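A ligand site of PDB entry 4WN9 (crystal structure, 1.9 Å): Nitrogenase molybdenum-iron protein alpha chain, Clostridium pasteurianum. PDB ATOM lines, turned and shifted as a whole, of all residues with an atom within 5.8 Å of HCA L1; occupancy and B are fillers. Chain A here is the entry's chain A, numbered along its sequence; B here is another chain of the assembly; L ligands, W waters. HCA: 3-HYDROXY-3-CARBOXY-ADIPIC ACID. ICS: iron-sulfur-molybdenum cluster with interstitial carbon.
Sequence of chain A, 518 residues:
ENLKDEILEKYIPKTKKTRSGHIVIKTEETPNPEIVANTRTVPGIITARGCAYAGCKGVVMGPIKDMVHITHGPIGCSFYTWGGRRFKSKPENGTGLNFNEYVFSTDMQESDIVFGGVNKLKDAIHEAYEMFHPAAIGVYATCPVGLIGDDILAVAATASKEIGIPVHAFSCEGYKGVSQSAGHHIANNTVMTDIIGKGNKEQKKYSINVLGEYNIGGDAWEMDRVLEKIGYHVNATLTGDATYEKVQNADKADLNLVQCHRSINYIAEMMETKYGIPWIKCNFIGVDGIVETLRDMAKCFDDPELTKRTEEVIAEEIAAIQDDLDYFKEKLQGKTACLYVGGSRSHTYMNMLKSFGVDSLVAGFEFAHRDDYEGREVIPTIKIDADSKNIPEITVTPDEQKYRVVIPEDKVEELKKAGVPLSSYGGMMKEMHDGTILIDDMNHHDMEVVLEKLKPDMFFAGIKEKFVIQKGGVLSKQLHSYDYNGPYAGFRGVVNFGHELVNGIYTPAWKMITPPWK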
ATOM      1  N   ALA A  48      20.541  17.100  12.369  1.00  0.00           N
ATOM      2  CA  ALA A  48      20.910  17.146  10.937  1.00  0.00           C
ATOM      3  C   ALA A  48      19.713  16.889   9.993  1.00  0.00           C
ATOM      4  O   ALA A  48      19.849  16.968   8.768  1.00  0.00           O
ATOM      5  CB  ALA A  48      22.012  16.132  10.651  1.00  0.00           C
ATOM      6  N   GLY A  50      16.151  16.355   7.888  1.00  0.00           N
ATOM      7  CA  GLY A  50      15.381  17.053   6.883  1.00  0.00           C
ATOM      8  C   GLY A  50      13.919  16.700   7.034  1.00  0.00           C
ATOM      9  O   GLY A  50      13.495  16.213   8.085  1.00  0.00           O
ATOM     10  N   ALA A  54      11.738  16.215   1.354  1.00  0.00           N
ATOM     11  CA  ALA A  54      13.075  15.811   0.896  1.00  0.00           C
ATOM     12  C   ALA A  54      13.160  14.304   0.677  1.00  0.00           C
ATOM     13  O   ALA A  54      13.761  13.845  -0.275  1.00  0.00           O
ATOM     14  CB  ALA A  54      14.154  16.231   1.910  1.00  0.00           C
ATOM     15  N   VAL A  59      14.602  12.523  -2.623  1.00  0.00           N
ATOM     16  CA  VAL A  59      15.358  11.250  -2.577  1.00  0.00           C
ATOM     17  C   VAL A  59      14.821  10.141  -3.503  1.00  0.00           C
ATOM     18  O   VAL A  59      15.566   9.624  -4.347  1.00  0.00           O
ATOM     19  CB  VAL A  59      15.436  10.696  -1.124  1.00  0.00           C
ATOM     20  CG1 VAL A  59      16.019   9.296  -1.121  1.00  0.00           C
ATOM     21  CG2 VAL A  59      16.266  11.608  -0.238  1.00  0.00           C
ATOM     22  N   GLY A  84      22.060  19.383  -5.428  1.00  0.00           N
ATOM     23  CA  GLY A  84      22.753  19.100  -4.208  1.00  0.00           C
ATOM     24  C   GLY A  84      22.932  17.622  -3.898  1.00  0.00           C
ATOM     25  O   GLY A  84      23.947  17.214  -3.295  1.00  0.00           O
ATOM     26  N   ARG A  85      21.922  16.811  -4.261  1.00  0.00           N
ATOM     27  CA  ARG A  85      22.015  15.361  -4.141  1.00  0.00           C
ATOM     28  C   ARG A  85      22.457  14.835  -5.523  1.00  0.00           C
ATOM     29  O   ARG A  85      21.799  15.076  -6.553  1.00  0.00           O
ATOM     30  CB  ARG A  85      20.671  14.779  -3.704  1.00  0.00           C
ATOM     31  CG  ARG A  85      20.689  13.268  -3.533  1.00  0.00           C
ATOM     32  CD  ARG A  85      19.493  12.762  -2.750  1.00  0.00           C
ATOM     33  NE  ARG A  85      19.356  11.296  -2.764  1.00  0.00           N
ATOM     34  CZ  ARG A  85      18.601  10.608  -3.624  1.00  0.00           C
ATOM     35  NH1 ARG A  85      18.532   9.290  -3.537  1.00  0.00           N
ATOM     36  NH2 ARG A  85      17.925  11.227  -4.580  1.00  0.00           N
ATOM     37  N   ARG A  86      23.578  14.119  -5.538  1.00  0.00           N
ATOM     38  CA  ARG A  86      24.286  13.824  -6.792  1.00  0.00           C
ATOM     39  C   ARG A  86      23.900  12.508  -7.510  1.00  0.00           C
ATOM     40  O   ARG A  86      24.784  11.732  -7.932  1.00  0.00           O
ATOM     41  CB  ARG A  86      25.785  13.832  -6.523  1.00  0.00           C
ATOM     42  CG  ARG A  86      26.309  15.096  -5.865  1.00  0.00           C
ATOM     43  CD  ARG A  86      27.783  14.957  -5.544  1.00  0.00           C
ATOM     44  NE  ARG A  86      28.529  14.563  -6.725  1.00  0.00           N
ATOM     45  CZ  ARG A  86      29.221  13.425  -6.844  1.00  0.00           C
ATOM     46  NH1 ARG A  86      29.844  13.153  -7.989  1.00  0.00           N
ATOM     47  NH2 ARG A  86      29.277  12.566  -5.832  1.00  0.00           N
ATOM     48  N   GLN A 180      12.990  12.694   6.952  1.00  0.00           N
ATOM     49  CA  GLN A 180      12.904  12.258   5.567  1.00  0.00           C
ATOM     50  C   GLN A 180      12.210  10.912   5.452  1.00  0.00           C
ATOM     51  O   GLN A 180      11.766  10.536   4.371  1.00  0.00           O
ATOM     52  CB  GLN A 180      14.299  12.087   4.940  1.00  0.00           C
ATOM     53  CG  GLN A 180      15.106  13.357   4.825  1.00  0.00           C
ATOM     54  CD  GLN A 180      15.986  13.585   6.033  1.00  0.00           C
ATOM     55  OE1 GLN A 180      15.522  13.570   7.177  1.00  0.00           O
ATOM     56  NE2 GLN A 180      17.278  13.781   5.789  1.00  0.00           N
ATOM     57  N   GLU A 366      20.497   9.194  11.196  1.00  0.00           N
ATOM     58  CA  GLU A 366      19.658  10.392  11.354  1.00  0.00           C
ATOM     59  C   GLU A 366      18.206  10.024  11.631  1.00  0.00           C
ATOM     60  O   GLU A 366      17.583  10.596  12.516  1.00  0.00           O
ATOM     61  CB  GLU A 366      19.578  11.184  10.057  1.00  0.00           C
ATOM     62  CG  GLU A 366      20.748  12.080   9.731  1.00  0.00           C
ATOM     63  CD  GLU A 366      20.513  12.781   8.405  1.00  0.00           C
ATOM     64  OE1 GLU A 366      21.340  12.586   7.504  1.00  0.00           O
ATOM     65  OE2 GLU A 366      19.493  13.496   8.259  1.00  0.00           O
ATOM     66  N   PHE A 367      17.665   9.140  10.795  1.00  0.00           N
ATOM     67  CA  PHE A 367      16.223   8.926  10.676  1.00  0.00           C
ATOM     68  C   PHE A 367      15.801   7.463  10.492  1.00  0.00           C
ATOM     69  O   PHE A 367      14.631   7.182  10.199  1.00  0.00           O
ATOM     70  CB  PHE A 367      15.671   9.749   9.508  1.00  0.00           C
ATOM     71  CG  PHE A 367      16.422   9.534   8.234  1.00  0.00           C
ATOM     72  CD1 PHE A 367      16.284   8.361   7.525  1.00  0.00           C
ATOM     73  CD2 PHE A 367      17.246  10.519   7.727  1.00  0.00           C
ATOM     74  CE1 PHE A 367      16.966   8.160   6.345  1.00  0.00           C
ATOM     75  CE2 PHE A 367      17.916  10.332   6.538  1.00  0.00           C
ATOM     76  CZ  PHE A 367      17.787   9.150   5.851  1.00  0.00           C
ATOM     77  N   ALA A 461      30.388  12.026   7.824  1.00  0.00           N
ATOM     78  CA  ALA A 461      29.029  12.484   8.003  1.00  0.00           C
ATOM     79  C   ALA A 461      28.622  13.257   6.767  1.00  0.00           C
ATOM     80  O   ALA A 461      28.786  12.743   5.643  1.00  0.00           O
ATOM     81  CB  ALA A 461      28.894  13.299   9.274  1.00  0.00           C
ATOM     82  N   GLY A 462      28.098  14.473   6.970  1.00  0.00           N
ATOM     83  CA  GLY A 462      27.545  15.245   5.861  1.00  0.00           C
ATOM     84  C   GLY A 462      28.136  16.638   5.773  1.00  0.00           C
ATOM     85  O   GLY A 462      29.178  16.953   6.387  1.00  0.00           O
ATOM     86  N   ILE A 463      27.479  17.493   5.010  1.00  0.00           N
ATOM     87  CA  ILE A 463      28.021  18.820   4.716  1.00  0.00           C
ATOM     88  C   ILE A 463      27.928  19.759   5.918  1.00  0.00           C
ATOM     89  O   ILE A 463      28.810  20.605   6.092  1.00  0.00           O
ATOM     90  CB  ILE A 463      27.373  19.418   3.454  1.00  0.00           C
ATOM     91  CG1 ILE A 463      28.075  20.719   3.041  1.00  0.00           C
ATOM     92  CG2 ILE A 463      25.871  19.602   3.641  1.00  0.00           C
ATOM     93  CD1 ILE A 463      29.455  20.513   2.447  1.00  0.00           C
ATOM     94  N   LYS A 464      26.901  19.588   6.755  1.00  0.00           N
ATOM     95  CA  LYS A 464      26.692  20.475   7.891  1.00  0.00           C
ATOM     96  C   LYS A 464      27.703  20.173   8.999  1.00  0.00           C
ATOM     97  O   LYS A 464      28.133  21.060   9.687  1.00  0.00           O
ATOM     98  CB  LYS A 464      25.249  20.406   8.429  1.00  0.00           C
ATOM     99  CG  LYS A 464      24.169  20.694   7.347  1.00  0.00           C
ATOM    100  CD  LYS A 464      22.774  20.818   7.946  1.00  0.00           C
ATOM    101  CE  LYS A 464      22.302  19.553   8.618  1.00  0.00           C
ATOM    102  NZ  LYS A 464      22.093  18.472   7.619  1.00  0.00           N
ATOM    103  N   GLU A 465      28.098  18.912   9.109  1.00  0.00           N
ATOM    104  CA  GLU A 465      29.088  18.527  10.111  1.00  0.00           C
ATOM    105  C   GLU A 465      30.523  18.676   9.619  1.00  0.00           C
ATOM    106  O   GLU A 465      31.411  18.968  10.405  1.00  0.00           O
ATOM    107  CB  GLU A 465      28.853  17.076  10.535  1.00  0.00           C
ATOM    108  CG  GLU A 465      27.485  16.838  11.120  1.00  0.00           C
ATOM    109  CD  GLU A 465      26.480  16.305  10.124  1.00  0.00           C
ATOM    110  OE1 GLU A 465      26.705  16.407   8.883  1.00  0.00           O
ATOM    111  OE2 GLU A 465      25.448  15.769  10.610  1.00  0.00           O
ATOM    112  N   GLN A 478      32.623  13.400   3.646  1.00  0.00           N
ATOM    113  CA  GLN A 478      31.189  13.246   3.404  1.00  0.00           C
ATOM    114  C   GLN A 478      30.838  11.916   2.779  1.00  0.00           C
ATOM    115  O   GLN A 478      31.406  11.539   1.771  1.00  0.00           O
ATOM    116  CB  GLN A 478      30.737  14.343   2.452  1.00  0.00           C
ATOM    117  CG  GLN A 478      30.904  15.761   2.978  1.00  0.00           C
ATOM    118  CD  GLN A 478      30.375  16.792   1.999  1.00  0.00           C
ATOM    119  OE1 GLN A 478      29.164  16.880   1.753  1.00  0.00           O
ATOM    120  NE2 GLN A 478      31.276  17.563   1.394  1.00  0.00           N
ATOM    121  N   HIS A 480      27.396  11.324   2.076  1.00  0.00           N
ATOM    122  CA  HIS A 480      26.220  11.521   1.209  1.00  0.00           C
ATOM    123  C   HIS A 480      26.713  11.923  -0.166  1.00  0.00           C
ATOM    124  O   HIS A 480      26.530  11.196  -1.141  1.00  0.00           O
ATOM    125  CB  HIS A 480      25.235  12.595   1.713  1.00  0.00           C
ATOM    126  CG  HIS A 480      24.849  12.481   3.152  1.00  0.00           C
ATOM    127  ND1 HIS A 480      23.567  12.157   3.550  1.00  0.00           N
ATOM    128  CD2 HIS A 480      25.563  12.660   4.273  1.00  0.00           C
ATOM    129  CE1 HIS A 480      23.521  12.166   4.866  1.00  0.00           C
ATOM    130  NE2 HIS A 480      24.711  12.456   5.333  1.00  0.00           N
ATOM    131  N   SER A 481      27.368  13.101  -0.246  1.00  0.00           N
ATOM    132  CA  SER A 481      27.880  13.623  -1.522  1.00  0.00           C
ATOM    133  C   SER A 481      29.245  13.072  -1.976  1.00  0.00           C
ATOM    134  O   SER A 481      29.730  13.461  -3.035  1.00  0.00           O
ATOM    135  CB  SER A 481      28.079  15.131  -1.431  1.00  0.00           C
ATOM    136  OG  SER A 481      29.174  15.385  -0.567  1.00  0.00           O
ATOM    137  N   SER B  50      17.829  22.827   7.790  1.00  0.00           N
ATOM    138  CA  SER B  50      18.911  22.056   7.223  1.00  0.00           C
ATOM    139  C   SER B  50      19.295  22.560   5.833  1.00  0.00           C
ATOM    140  O   SER B  50      20.471  22.740   5.534  1.00  0.00           O
ATOM    141  CB  SER B  50      18.554  20.579   7.163  1.00  0.00           C
ATOM    142  OG  SER B  50      19.657  19.821   6.682  1.00  0.00           O
ATOM    143  N   TYR B  51      18.310  22.825   4.982  1.00  0.00           N
ATOM    144  CA  TYR B  51      18.574  23.321   3.626  1.00  0.00           C
ATOM    145  C   TYR B  51      19.282  24.654   3.632  1.00  0.00           C
ATOM    146  O   TYR B  51      20.135  24.906   2.812  1.00  0.00           O
ATOM    147  CB  TYR B  51      17.282  23.497   2.838  1.00  0.00           C
ATOM    148  CG  TYR B  51      16.721  22.258   2.223  1.00  0.00           C
ATOM    149  CD1 TYR B  51      17.554  21.220   1.820  1.00  0.00           C
ATOM    150  CD2 TYR B  51      15.339  22.151   1.962  1.00  0.00           C
ATOM    151  CE1 TYR B  51      17.032  20.102   1.208  1.00  0.00           C
ATOM    152  CE2 TYR B  51      14.818  21.032   1.349  1.00  0.00           C
ATOM    153  CZ  TYR B  51      15.672  20.015   0.975  1.00  0.00           C
ATOM    154  OH  TYR B  51      15.173  18.892   0.370  1.00  0.00           O
ATOM    155  N   THR B  54      22.849  24.353   4.964  1.00  0.00           N
ATOM    156  CA  THR B  54      23.627  23.680   3.917  1.00  0.00           C
ATOM    157  C   THR B  54      24.108  24.623   2.803  1.00  0.00           C
ATOM    158  O   THR B  54      25.263  24.561   2.398  1.00  0.00           O
ATOM    159  CB  THR B  54      22.808  22.534   3.291  1.00  0.00           C
ATOM    160  OG1 THR B  54      22.548  21.546   4.286  1.00  0.00           O
ATOM    161  CG2 THR B  54      23.536  21.895   2.155  1.00  0.00           C
ATOM    162  N   ARG B  58      27.911  25.246   1.734  1.00  0.00           N
ATOM    163  CA  ARG B  58      28.389  24.981   0.376  1.00  0.00           C
ATOM    164  C   ARG B  58      29.030  26.194  -0.309  1.00  0.00           C
ATOM    165  O   ARG B  58      29.982  26.044  -1.094  1.00  0.00           O
ATOM    166  CB  ARG B  58      27.240  24.502  -0.476  1.00  0.00           C
ATOM    167  CG  ARG B  58      26.774  23.097  -0.108  1.00  0.00           C
ATOM    168  CD  ARG B  58      25.541  22.714  -0.902  1.00  0.00           C
ATOM    169  NE  ARG B  58      25.255  21.299  -0.701  1.00  0.00           N
ATOM    170  CZ  ARG B  58      24.078  20.741  -0.871  1.00  0.00           C
ATOM    171  NH1 ARG B  58      23.037  21.465  -1.277  1.00  0.00           N
ATOM    172  NH2 ARG B  58      23.934  19.448  -0.618  1.00  0.00           N
HETATM  173  C1  HCA L   1      18.755  15.374   2.295  1.00  0.00           C
HETATM  174  C2  HCA L   1      19.785  15.063   1.234  1.00  0.00           C
HETATM  175  C3  HCA L   1      21.142  14.683   1.839  1.00  0.00           C
HETATM  176  C4  HCA L   1      21.861  15.833   2.538  1.00  0.00           C
HETATM  177  C5  HCA L   1      23.333  15.448   2.697  1.00  0.00           C
HETATM  178  C6  HCA L   1      24.229  16.280   3.601  1.00  0.00           C
HETATM  179  C7  HCA L   1      22.006  14.223   0.691  1.00  0.00           C
HETATM  180  O1  HCA L   1      18.608  14.580   3.243  1.00  0.00           O
HETATM  181  O2  HCA L   1      18.068  16.412   2.196  1.00  0.00           O
HETATM  182  O3  HCA L   1      25.433  16.363   3.246  1.00  0.00           O
HETATM  183  O4  HCA L   1      23.810  16.801   4.662  1.00  0.00           O
HETATM  184  O5  HCA L   1      22.512  13.089   0.717  1.00  0.00           O
HETATM  185  O6  HCA L   1      22.227  15.026  -0.248  1.00  0.00           O
HETATM  186  O7  HCA L   1      20.954  13.624   2.787  1.00  0.00           O
HETATM  187 FE1  ICS L   2      18.865   5.362   1.689  1.00  0.00          FE
HETATM  188 MO1  ICS L   2      21.683  11.696   2.136  1.00  0.00          MO
HETATM  189 FE2  ICS L   2      18.389   7.907   2.249  1.00  0.00          FE
HETATM  190 FE3  ICS L   2      20.079   7.270   0.279  1.00  0.00          FE
HETATM  191 FE4  ICS L   2      20.739   6.797   2.802  1.00  0.00          FE
HETATM  192 FE5  ICS L   2      21.749   9.153   2.978  1.00  0.00          FE
HETATM  193 FE6  ICS L   2      19.439  10.267   2.379  1.00  0.00          FE
HETATM  194 FE7  ICS L   2      21.111   9.659   0.502  1.00  0.00          FE
HETATM  195  CX  ICS L   2      20.270   8.470   1.892  1.00  0.00           C
HETATM  196  S1A ICS L   2      18.727   6.267   3.762  1.00  0.00           S
HETATM  197  S1B ICS L   2      20.747  10.831   4.085  1.00  0.00           S
HETATM  198  S2A ICS L   2      17.846   6.842   0.325  1.00  0.00           S
HETATM  199  S2B ICS L   2      17.338   9.811   2.785  1.00  0.00           S
HETATM  200  S3A ICS L   2      22.457   7.298   4.063  1.00  0.00           S
HETATM  201  S3B ICS L   2      19.870  11.533   0.615  1.00  0.00           S
HETATM  202  S4A ICS L   2      21.089   5.391   1.054  1.00  0.00           S
HETATM  203  S4B ICS L   2      23.119  10.002   1.416  1.00  0.00           S
HETATM  204  S5A ICS L   2      21.078   8.428  -1.354  1.00  0.00           S
HETATM  205  O   HOH W   1      17.746  17.756   4.226  1.00  0.00           O
HETATM  206  O   HOH W   2      25.832  17.569   0.636  1.00  0.00           O
HETATM  207  O   HOH W   3      27.613  14.780   2.280  1.00  0.00           O
HETATM  208  O   HOH W   4      16.833  16.913  -0.460  1.00  0.00           O
HETATM  209  O   HOH W   5      20.594  14.014   5.520  1.00  0.00           O
HETATM  210  O   HOH W   6      21.413  17.652  -0.899  1.00  0.00           O
HETATM  211  O   HOH W   7      22.168  18.882   4.626  1.00  0.00           O
HETATM  212  O   HOH W   8      24.898  17.483   7.094  1.00  0.00           O
HETATM  213  O   HOH W   9      23.335  11.707  -1.517  1.00  0.00           O
HETATM  214  O   HOH W  10      24.597  15.567  -1.329  1.00  0.00           O
HETATM  215  O   HOH W  11      22.370  15.746   6.733  1.00  0.00           O
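ND1 of His 480 lies close to O7 of HCA L1.
Ala 54 of chain A touches HCA L1 (CB to O2, 3.9 Å).
Arg 85 touches HCA L1.
CA of Gly 462 touches O3 of HCA L1 (3.5 Å).
Tyr 51 of chain B touches HCA L1.
Hydrophobic or aromatic side chains that line HCA L1: Ala 54 of chain A, Ile 463, His 480 and Tyr 51 of chain B.
Along chain A the residues within 4 Å of HCA L1 span positions 54 to 480.
The backbone carbonyl oxygen (O) of Val 59 lies within hydrogen-bond range of the guanidinium group (NH2) of Arg 85.
The side-chain amide nitrogen of Gln 180 is in hydrogen-bond range of the side-chain carboxylate of Glu 366, 3.3 Å away.
The backbone NH (N) of Gly 462 sits at hydrogen-bond distance from the side-chain carboxylate (OE1) of Glu 465 (3.1 Å).
The side-chain amide oxygen (OE1) of Gln 180 is in hydrogen-bond range of the backbone NH (N) of Gly 50 of chain A, 2.9 Å away.
OG of Ser 50 of chain B is in hydrogen-bond range of NZ of Lys 464.
The side-chain amino group (NZ) of Lys 464 lies within hydrogen-bond range of the backbone carbonyl oxygen (O) of Ala 48, 2.9 Å away.
The backbone NH (N) of Val 59 lies within hydrogen-bond range of the backbone carbonyl oxygen (O) of Ala 54 of chain A, at 2.8 Å.
Water W7 lies within hydrogen-bond range of an oxygen (O4) of HCA L1 (2.7 Å), the side-chain hydroxyl of Thr 54 of chain B (2.7 Å), the side-chain amino group of Lys 464 (3.0 Å) and the side-chain hydroxyl of Ser 50 of chain B (3.4 Å).
Water W11 lies within hydrogen-bond range of O4 of HCA L1 (2.7 Å), NZ of Lys 464 (2.9 Å), OE1 of Glu 366 (3.4 Å) and O of Ala 48 (3.5 Å).
Water W5 lies within hydrogen-bond range of OE1 of Glu 366 (2.6 Å), O1 of HCA L1 (3.1 Å), NE2 of Gln 180 (3.3 Å) and S1B of ICS L2 (3.5 Å).
Water W6 lies within hydrogen-bond range of O6 of HCA L1 (2.8 Å) and NH2 of Arg 58 of chain B (3.1 Å).
Water W3 lies within hydrogen-bond range of OE1 of Gln 478, O3 of HCA L1, N of Ser 481 and N of His 480.
Water W4 lies within hydrogen-bond range of OH of Tyr 51 of chain B and O2 of HCA L1.
An oxygen (O5) of HCA L1 binds a molybdenum atom (MO1) of ICS L2 (2.2 Å).
The backbone NH (N) of Ile 463 sits at hydrogen-bond distance from an oxygen (O3) of HCA L1 (2.9 Å).
The guanidinium group (NE) of Arg 85 lies close to a sulfur (S3B) of ICS L2, 3.4 Å away.
MO1 of ICS L2 is bound by ND1 of His 480, 2.4 Å away.
The side-chain amide nitrogen of Gln 180 sits at hydrogen-bond distance from an oxygen (O1) of HCA L1, at 3.0 Å.
NZ of Lys 464 lies within salt-bridge range of O4 of HCA L1 (3.8 Å).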
